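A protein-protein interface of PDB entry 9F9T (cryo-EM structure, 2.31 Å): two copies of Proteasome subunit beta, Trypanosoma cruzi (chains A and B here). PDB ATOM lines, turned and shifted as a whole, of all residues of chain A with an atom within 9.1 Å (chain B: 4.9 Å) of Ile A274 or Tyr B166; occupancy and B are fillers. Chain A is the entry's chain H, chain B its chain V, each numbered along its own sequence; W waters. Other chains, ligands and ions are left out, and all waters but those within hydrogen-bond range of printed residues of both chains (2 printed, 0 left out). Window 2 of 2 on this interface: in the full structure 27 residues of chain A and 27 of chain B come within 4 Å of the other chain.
NE2 of Gln A264 is in hydrogen-bond range of O of Cys B174, 3.3 Å away. The backbone NH (N) of Lys B176 is in hydrogen-bond range of the side-chain amide oxygen (OE1) of Gln A264 (3.0 Å). The backbone NH (N) of Ile A274 lies within hydrogen-bond range of the side-chain amide oxygen (OD1) of Asn B161 (3.1 Å).
The backbone carbonyl oxygen (O) of Ala A262 is in hydrogen-bond range of the side-chain amide nitrogen (ND2) of Asn A277 (2.8 Å). N of Gln A264 lies within hydrogen-bond range of OD1 of Asn A277 (3.2 Å). The side-chain hydroxyl of Ser A271 is in hydrogen-bond range of the backbone NH of Lys A273 (2.8 Å). The backbone carbonyl oxygen (O) of Val B154 sits at hydrogen-bond distance from the backbone NH (N) of Tyr B166. N of Ser B167 sits at hydrogen-bond distance from O of Val B175 (2.9 Å).
Ala A262 touches Lys B176 (CB to O, 3.5 Å). OE1 of Gln A264 touches CA of Val B175, at 3.5 Å. Asn B161 touches Ala A272. CG of Lys A273 touches OD1 of Asn B161 (3.6 Å). Tyr B166 touches Ile A274 (OH to CD1, 3.8 Å).
Of the printed residues of chain B, Ala A262 touches Lys B176 (3.5 Å). Pro A267 touches none of the printed residues of chain B. Ile A274 touches just these residues of chain B: Asn B161 and Tyr B166. Thr A275 touches none of the printed residues of chain B. No residue of chain A comes within 4 Å of Val B154. No residue of chain A comes within 4 Å of Val B165. Printed residues of chain A within 4 Å of Cys B174: Gln A264. Of the printed residues of chain A, Val B175 touches Gln A264 (3.5 Å). Of the printed residues of chain A, Lys B176 touches Ala A262 and Gln A264. The nearest residue of chain A that does not touch Tyr B166 is Gln A264 (5.9 Å). The nearest printed residue of chain B that does not touch Gln A264 is Tyr B166 (5.9 Å).
Among the printed residues, 8 pairs touch across the chains. Among the printed residues, no Asp or Glu carboxylate lies within 4 Å of a Lys or Arg side-chain nitrogen of the other chain.
No position is printed for both chains.
Water W1 lies within hydrogen-bond range of O of Lys B176 (2.7 Å) and N of Val A263 (3.2 Å). Water W2 bridges OE1 of Gln A264 and O of Cys B174.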
ATOM      1  N   LEU A 261     -22.756   2.587   6.594  1.00  0.00           N
ATOM      2  CA  LEU A 261     -21.786   1.560   6.928  1.00  0.00           C
ATOM      3  C   LEU A 261     -20.556   2.190   7.556  1.00  0.00           C
ATOM      4  O   LEU A 261     -20.133   3.258   7.147  1.00  0.00           O
ATOM      5  CB  LEU A 261     -21.360   0.775   5.683  1.00  0.00           C
ATOM      6  CG  LEU A 261     -22.403  -0.130   5.036  1.00  0.00           C
ATOM      7  CD1 LEU A 261     -21.889  -0.739   3.753  1.00  0.00           C
ATOM      8  CD2 LEU A 261     -22.871  -1.228   5.965  1.00  0.00           C
ATOM      9  N   ALA A 262     -19.906   1.445   8.452  1.00  0.00           N
ATOM     10  CA  ALA A 262     -18.672   1.878   9.059  1.00  0.00           C
ATOM     11  C   ALA A 262     -17.628   2.047   8.003  1.00  0.00           C
ATOM     12  O   ALA A 262     -17.512   1.152   7.171  1.00  0.00           O
ATOM     13  CB  ALA A 262     -18.107   0.833   9.960  1.00  0.00           C
ATOM     14  N   VAL A 263     -16.744   3.017   8.214  1.00  0.00           N
ATOM     15  CA  VAL A 263     -15.730   3.320   7.252  1.00  0.00           C
ATOM     16  C   VAL A 263     -14.464   2.540   7.559  1.00  0.00           C
ATOM     17  O   VAL A 263     -13.481   3.064   8.063  1.00  0.00           O
ATOM     18  CB  VAL A 263     -15.533   4.820   7.178  1.00  0.00           C
ATOM     19  CG1 VAL A 263     -14.584   5.141   6.038  1.00  0.00           C
ATOM     20  CG2 VAL A 263     -16.866   5.491   6.914  1.00  0.00           C
ATOM     21  N   GLN A 264     -14.526   1.259   7.194  1.00  0.00           N
ATOM     22  CA  GLN A 264     -13.436   0.321   7.333  1.00  0.00           C
ATOM     23  C   GLN A 264     -12.545   0.258   6.103  1.00  0.00           C
ATOM     24  O   GLN A 264     -11.465  -0.307   6.196  1.00  0.00           O
ATOM     25  CB  GLN A 264     -14.063  -1.033   7.556  1.00  0.00           C
ATOM     26  CG  GLN A 264     -14.814  -1.089   8.866  1.00  0.00           C
ATOM     27  CD  GLN A 264     -13.840  -0.920  10.009  1.00  0.00           C
ATOM     28  OE1 GLN A 264     -13.702   0.153  10.597  1.00  0.00           O
ATOM     29  NE2 GLN A 264     -13.086  -1.988  10.250  1.00  0.00           N
ATOM     30  N   ASN A 265     -13.016   0.769   4.949  1.00  0.00           N
ATOM     31  CA  ASN A 265     -12.356   0.496   3.689  1.00  0.00           C
ATOM     32  C   ASN A 265     -12.175   1.782   2.914  1.00  0.00           C
ATOM     33  O   ASN A 265     -12.607   1.915   1.785  1.00  0.00           O
ATOM     34  CB  ASN A 265     -13.105  -0.550   2.868  1.00  0.00           C
ATOM     35  CG  ASN A 265     -13.258  -1.931   3.496  1.00  0.00           C
ATOM     36  OD1 ASN A 265     -12.496  -2.371   4.350  1.00  0.00           O
ATOM     37  ND2 ASN A 265     -14.347  -2.597   3.178  1.00  0.00           N
ATOM     38  N   PRO A 266     -11.504   2.795   3.482  1.00  0.00           N
ATOM     39  CA  PRO A 266     -11.277   4.044   2.764  1.00  0.00           C
ATOM     40  C   PRO A 266     -10.301   3.859   1.612  1.00  0.00           C
ATOM     41  O   PRO A 266      -9.413   3.012   1.675  1.00  0.00           O
ATOM     42  CB  PRO A 266     -10.611   4.882   3.878  1.00  0.00           C
ATOM     43  CG  PRO A 266      -9.778   3.864   4.656  1.00  0.00           C
ATOM     44  CD  PRO A 266     -10.788   2.747   4.771  1.00  0.00           C
ATOM     45  N   PRO A 267     -10.428   4.662   0.540  1.00  0.00           N
ATOM     46  CA  PRO A 267      -9.520   4.586  -0.591  1.00  0.00           C
ATOM     47  C   PRO A 267      -8.138   5.091  -0.242  1.00  0.00           C
ATOM     48  O   PRO A 267      -7.982   6.016   0.561  1.00  0.00           O
ATOM     49  CB  PRO A 267      -9.962   5.648  -1.605  1.00  0.00           C
ATOM     50  CG  PRO A 267     -11.147   6.363  -0.993  1.00  0.00           C
ATOM     51  CD  PRO A 267     -11.452   5.700   0.345  1.00  0.00           C
ATOM     52  N   SER A 269      -5.319   7.352  -0.398  1.00  0.00           N
ATOM     53  CA  SER A 269      -5.458   8.794  -0.511  1.00  0.00           C
ATOM     54  C   SER A 269      -4.205   9.511  -0.064  1.00  0.00           C
ATOM     55  O   SER A 269      -3.352   8.951   0.618  1.00  0.00           O
ATOM     56  CB  SER A 269      -6.615   9.311   0.311  1.00  0.00           C
ATOM     57  OG  SER A 269      -6.279   9.212   1.674  1.00  0.00           O
ATOM     58  N   SER A 271      -4.368  12.081   1.957  1.00  0.00           N
ATOM     59  CA  SER A 271      -4.792  12.801   3.162  1.00  0.00           C
ATOM     60  C   SER A 271      -5.143  11.787   4.227  1.00  0.00           C
ATOM     61  O   SER A 271      -5.624  10.710   3.927  1.00  0.00           O
ATOM     62  CB  SER A 271      -5.972  13.713   2.954  1.00  0.00           C
ATOM     63  OG  SER A 271      -6.609  14.099   4.212  1.00  0.00           O
ATOM     64  N   ALA A 272      -4.962  12.147   5.493  1.00  0.00           N
ATOM     65  CA  ALA A 272      -5.373  11.247   6.568  1.00  0.00           C
ATOM     66  C   ALA A 272      -6.872  11.370   6.825  1.00  0.00           C
ATOM     67  O   ALA A 272      -7.422  10.511   7.489  1.00  0.00           O
ATOM     68  CB  ALA A 272      -4.554  11.507   7.815  1.00  0.00           C
ATOM     69  N   LYS A 273      -7.531  12.344   6.198  1.00  0.00           N
ATOM     70  CA  LYS A 273      -8.965  12.486   6.325  1.00  0.00           C
ATOM     71  C   LYS A 273      -9.748  11.263   5.827  1.00  0.00           C
ATOM     72  O   LYS A 273      -9.544  10.757   4.733  1.00  0.00           O
ATOM     73  CB  LYS A 273      -9.454  13.750   5.624  1.00  0.00           C
ATOM     74  CG  LYS A 273     -10.886  14.072   5.964  1.00  0.00           C
ATOM     75  CD  LYS A 273     -11.422  15.354   5.348  1.00  0.00           C
ATOM     76  CE  LYS A 273     -12.825  15.712   5.832  1.00  0.00           C
ATOM     77  NZ  LYS A 273     -13.151  15.075   7.145  1.00  0.00           N
ATOM     78  N   ILE A 274     -10.711  10.850   6.648  1.00  0.00           N
ATOM     79  CA  ILE A 274     -11.570   9.704   6.398  1.00  0.00           C
ATOM     80  C   ILE A 274     -12.971  10.199   6.091  1.00  0.00           C
ATOM     81  O   ILE A 274     -13.493  11.032   6.823  1.00  0.00           O
ATOM     82  CB  ILE A 274     -11.591   8.800   7.640  1.00  0.00           C
ATOM     83  CG1 ILE A 274     -10.251   8.090   7.842  1.00  0.00           C
ATOM     84  CG2 ILE A 274     -12.775   7.842   7.599  1.00  0.00           C
ATOM     85  CD1 ILE A 274      -9.995   7.697   9.267  1.00  0.00           C
ATOM     86  N   THR A 275     -13.581   9.608   5.055  1.00  0.00           N
ATOM     87  CA  THR A 275     -14.791  10.143   4.459  1.00  0.00           C
ATOM     88  C   THR A 275     -15.796   9.012   4.202  1.00  0.00           C
ATOM     89  O   THR A 275     -16.821   8.910   4.878  1.00  0.00           O
ATOM     90  CB  THR A 275     -14.432  10.957   3.199  1.00  0.00           C
ATOM     91  OG1 THR A 275     -13.190  10.521   2.630  1.00  0.00           O
ATOM     92  CG2 THR A 275     -14.340  12.441   3.487  1.00  0.00           C
ATOM     93  N   VAL A 276     -15.481   8.185   3.196  1.00  0.00           N
ATOM     94  CA  VAL A 276     -16.366   7.145   2.708  1.00  0.00           C
ATOM     95  C   VAL A 276     -15.570   5.870   2.422  1.00  0.00           C
ATOM     96  O   VAL A 276     -14.355   5.896   2.292  1.00  0.00           O
ATOM     97  CB  VAL A 276     -17.119   7.620   1.456  1.00  0.00           C
ATOM     98  CG1 VAL A 276     -17.946   8.837   1.783  1.00  0.00           C
ATOM     99  CG2 VAL A 276     -16.186   7.902   0.296  1.00  0.00           C
ATOM    100  N   ASN A 277     -16.291   4.750   2.410  1.00  0.00           N
ATOM    101  CA  ASN A 277     -15.770   3.496   1.924  1.00  0.00           C
ATOM    102  C   ASN A 277     -15.562   3.591   0.408  1.00  0.00           C
ATOM    103  O   ASN A 277     -16.357   4.197  -0.311  1.00  0.00           O
ATOM    104  CB  ASN A 277     -16.721   2.371   2.304  1.00  0.00           C
ATOM    105  CG  ASN A 277     -16.641   1.962   3.761  1.00  0.00           C
ATOM    106  OD1 ASN A 277     -15.579   1.529   4.213  1.00  0.00           O
ATOM    107  ND2 ASN A 277     -17.762   1.975   4.475  1.00  0.00           N
ATOM    108  N   VAL B 130      -6.646  10.732  15.803  1.00  0.00           N
ATOM    109  CA  VAL B 130      -7.117   9.616  16.567  1.00  0.00           C
ATOM    110  C   VAL B 130      -6.719   8.312  15.886  1.00  0.00           C
ATOM    111  O   VAL B 130      -6.257   7.368  16.542  1.00  0.00           O
ATOM    112  CB  VAL B 130      -8.607   9.691  16.866  1.00  0.00           C
ATOM    113  CG1 VAL B 130      -9.002   8.452  17.632  1.00  0.00           C
ATOM    114  CG2 VAL B 130      -8.953  10.939  17.641  1.00  0.00           C
ATOM    115  N   THR B 131      -6.759   8.323  14.561  1.00  0.00           N
ATOM    116  CA  THR B 131      -6.524   7.111  13.778  1.00  0.00           C
ATOM    117  C   THR B 131      -5.130   6.567  14.007  1.00  0.00           C
ATOM    118  O   THR B 131      -4.963   5.369  14.127  1.00  0.00           O
ATOM    119  CB  THR B 131      -6.851   7.354  12.308  1.00  0.00           C
ATOM    120  OG1 THR B 131      -6.460   6.333  11.403  1.00  0.00           O
ATOM    121  CG2 THR B 131      -6.055   8.556  11.894  1.00  0.00           C
ATOM    122  N   ALA B 134      -5.134   4.832  17.345  1.00  0.00           N
ATOM    123  CA  ALA B 134      -5.849   3.607  17.209  1.00  0.00           C
ATOM    124  C   ALA B 134      -4.992   2.577  16.513  1.00  0.00           C
ATOM    125  O   ALA B 134      -4.915   1.461  17.006  1.00  0.00           O
ATOM    126  CB  ALA B 134      -7.150   3.844  16.502  1.00  0.00           C
ATOM    127  N   ILE B 152     -10.080  -2.887  24.166  1.00  0.00           N
ATOM    128  CA  ILE B 152      -9.719  -1.478  24.237  1.00  0.00           C
ATOM    129  C   ILE B 152     -10.694  -0.653  23.414  1.00  0.00           C
ATOM    130  O   ILE B 152     -11.221  -1.132  22.453  1.00  0.00           O
ATOM    131  CB  ILE B 152      -8.287  -1.323  23.695  1.00  0.00           C
ATOM    132  CG1 ILE B 152      -7.268  -2.034  24.567  1.00  0.00           C
ATOM    133  CG2 ILE B 152      -7.895   0.126  23.583  1.00  0.00           C
ATOM    134  CD1 ILE B 152      -7.151  -1.389  25.959  1.00  0.00           C
ATOM    135  N   ILE B 153     -10.924   0.571  23.827  1.00  0.00           N
ATOM    136  CA  ILE B 153     -11.607   1.564  23.046  1.00  0.00           C
ATOM    137  C   ILE B 153     -10.732   2.781  23.021  1.00  0.00           C
ATOM    138  O   ILE B 153     -10.243   3.158  24.047  1.00  0.00           O
ATOM    139  CB  ILE B 153     -12.960   1.879  23.658  1.00  0.00           C
ATOM    140  CG1 ILE B 153     -13.817   0.639  23.677  1.00  0.00           C
ATOM    141  CG2 ILE B 153     -13.692   2.980  22.925  1.00  0.00           C
ATOM    142  CD1 ILE B 153     -15.089   0.829  24.404  1.00  0.00           C
ATOM    143  N   VAL B 154     -10.392   3.257  21.837  1.00  0.00           N
ATOM    144  CA  VAL B 154      -9.638   4.480  21.683  1.00  0.00           C
ATOM    145  C   VAL B 154     -10.577   5.503  21.164  1.00  0.00           C
ATOM    146  O   VAL B 154     -11.348   5.155  20.313  1.00  0.00           O
ATOM    147  CB  VAL B 154      -8.522   4.286  20.708  1.00  0.00           C
ATOM    148  CG1 VAL B 154      -7.831   5.578  20.317  1.00  0.00           C
ATOM    149  CG2 VAL B 154      -7.525   3.277  21.223  1.00  0.00           C
ATOM    150  N   ASN B 161     -10.617  15.048  11.564  1.00  0.00           N
ATOM    151  CA  ASN B 161     -11.763  14.154  11.531  1.00  0.00           C
ATOM    152  C   ASN B 161     -12.744  14.299  12.685  1.00  0.00           C
ATOM    153  O   ASN B 161     -13.617  13.462  12.819  1.00  0.00           O
ATOM    154  CB  ASN B 161     -11.270  12.709  11.567  1.00  0.00           C
ATOM    155  CG  ASN B 161     -10.639  12.310  10.254  1.00  0.00           C
ATOM    156  OD1 ASN B 161     -11.201  12.578   9.204  1.00  0.00           O
ATOM    157  ND2 ASN B 161      -9.461  11.725  10.296  1.00  0.00           N
ATOM    158  N   SER B 164     -13.738  10.647  17.160  1.00  0.00           N
ATOM    159  CA  SER B 164     -13.824   9.325  16.599  1.00  0.00           C
ATOM    160  C   SER B 164     -13.633   8.272  17.628  1.00  0.00           C
ATOM    161  O   SER B 164     -13.024   8.465  18.625  1.00  0.00           O
ATOM    162  CB  SER B 164     -12.842   9.146  15.595  1.00  0.00           C
ATOM    163  OG  SER B 164     -12.582  10.400  14.980  1.00  0.00           O
ATOM    164  N   VAL B 165     -14.150   7.130  17.330  1.00  0.00           N
ATOM    165  CA  VAL B 165     -14.230   6.040  18.264  1.00  0.00           C
ATOM    166  C   VAL B 165     -13.752   4.806  17.511  1.00  0.00           C
ATOM    167  O   VAL B 165     -14.347   4.472  16.519  1.00  0.00           O
ATOM    168  CB  VAL B 165     -15.690   5.830  18.766  1.00  0.00           C
ATOM    169  CG1 VAL B 165     -15.721   4.687  19.744  1.00  0.00           C
ATOM    170  CG2 VAL B 165     -16.330   7.008  19.435  1.00  0.00           C
ATOM    171  N   TYR B 166     -12.786   4.101  18.057  1.00  0.00           N
ATOM    172  CA  TYR B 166     -12.394   2.817  17.563  1.00  0.00           C
ATOM    173  C   TYR B 166     -12.566   1.779  18.641  1.00  0.00           C
ATOM    174  O   TYR B 166     -12.143   2.038  19.737  1.00  0.00           O
ATOM    175  CB  TYR B 166     -10.930   2.827  17.194  1.00  0.00           C
ATOM    176  CG  TYR B 166     -10.693   3.736  16.024  1.00  0.00           C
ATOM    177  CD1 TYR B 166     -10.464   5.094  16.198  1.00  0.00           C
ATOM    178  CD2 TYR B 166     -10.748   3.274  14.717  1.00  0.00           C
ATOM    179  CE1 TYR B 166     -10.254   5.947  15.132  1.00  0.00           C
ATOM    180  CE2 TYR B 166     -10.632   4.156  13.648  1.00  0.00           C
ATOM    181  CZ  TYR B 166     -10.334   5.466  13.853  1.00  0.00           C
ATOM    182  OH  TYR B 166     -10.132   6.300  12.784  1.00  0.00           O
ATOM    183  N   SER B 167     -13.194   0.660  18.318  1.00  0.00           N
ATOM    184  CA  SER B 167     -13.169  -0.543  19.118  1.00  0.00           C
ATOM    185  C   SER B 167     -11.977  -1.423  18.733  1.00  0.00           C
ATOM    186  O   SER B 167     -11.648  -1.638  17.579  1.00  0.00           O
ATOM    187  CB  SER B 167     -14.367  -1.282  18.873  1.00  0.00           C
ATOM    188  OG  SER B 167     -14.631  -2.239  19.894  1.00  0.00           O
ATOM    189  N   ILE B 168     -11.271  -1.907  19.712  1.00  0.00           N
ATOM    190  CA  ILE B 168     -10.239  -2.866  19.429  1.00  0.00           C
ATOM    191  C   ILE B 168     -10.447  -4.023  20.381  1.00  0.00           C
ATOM    192  O   ILE B 168      -9.747  -4.124  21.371  1.00  0.00           O
ATOM    193  CB  ILE B 168      -8.879  -2.213  19.612  1.00  0.00           C
ATOM    194  CG1 ILE B 168      -8.754  -0.934  18.802  1.00  0.00           C
ATOM    195  CG2 ILE B 168      -7.742  -3.131  19.282  1.00  0.00           C
ATOM    196  CD1 ILE B 168      -7.477  -0.282  19.002  1.00  0.00           C
ATOM    197  N   CYS B 174      -9.756  -3.832  14.412  1.00  0.00           N
ATOM    198  CA  CYS B 174      -9.993  -2.443  14.727  1.00  0.00           C
ATOM    199  C   CYS B 174     -11.078  -1.853  13.865  1.00  0.00           C
ATOM    200  O   CYS B 174     -10.861  -1.643  12.682  1.00  0.00           O
ATOM    201  CB  CYS B 174      -8.744  -1.628  14.452  1.00  0.00           C
ATOM    202  SG  CYS B 174      -8.994   0.161  14.666  1.00  0.00           S
ATOM    203  N   VAL B 175     -12.136  -1.451  14.526  1.00  0.00           N
ATOM    204  CA  VAL B 175     -13.378  -1.036  13.906  1.00  0.00           C
ATOM    205  C   VAL B 175     -13.761   0.369  14.318  1.00  0.00           C
ATOM    206  O   VAL B 175     -13.795   0.688  15.490  1.00  0.00           O
ATOM    207  CB  VAL B 175     -14.496  -2.035  14.289  1.00  0.00           C
ATOM    208  CG1 VAL B 175     -15.802  -1.662  13.651  1.00  0.00           C
ATOM    209  CG2 VAL B 175     -14.092  -3.433  13.852  1.00  0.00           C
ATOM    210  N   LYS B 176     -14.176   1.155  13.336  1.00  0.00           N
ATOM    211  CA  LYS B 176     -14.430   2.566  13.515  1.00  0.00           C
ATOM    212  C   LYS B 176     -15.927   2.796  13.546  1.00  0.00           C
ATOM    213  O   LYS B 176     -16.569   2.639  12.534  1.00  0.00           O
ATOM    214  CB  LYS B 176     -13.824   3.427  12.418  1.00  0.00           C
ATOM    215  CG  LYS B 176     -14.072   4.939  12.544  1.00  0.00           C
ATOM    216  CD  LYS B 176     -13.369   5.744  11.492  1.00  0.00           C
ATOM    217  CE  LYS B 176     -13.365   7.269  11.624  1.00  0.00           C
ATOM    218  NZ  LYS B 176     -14.659   7.753  12.164  1.00  0.00           N
HETATM  219  O   HOH W   1     -17.209   4.683  10.930  1.00  0.00           O
HETATM  220  O   HOH W   2     -11.185   1.226  11.089  1.00  0.00           O
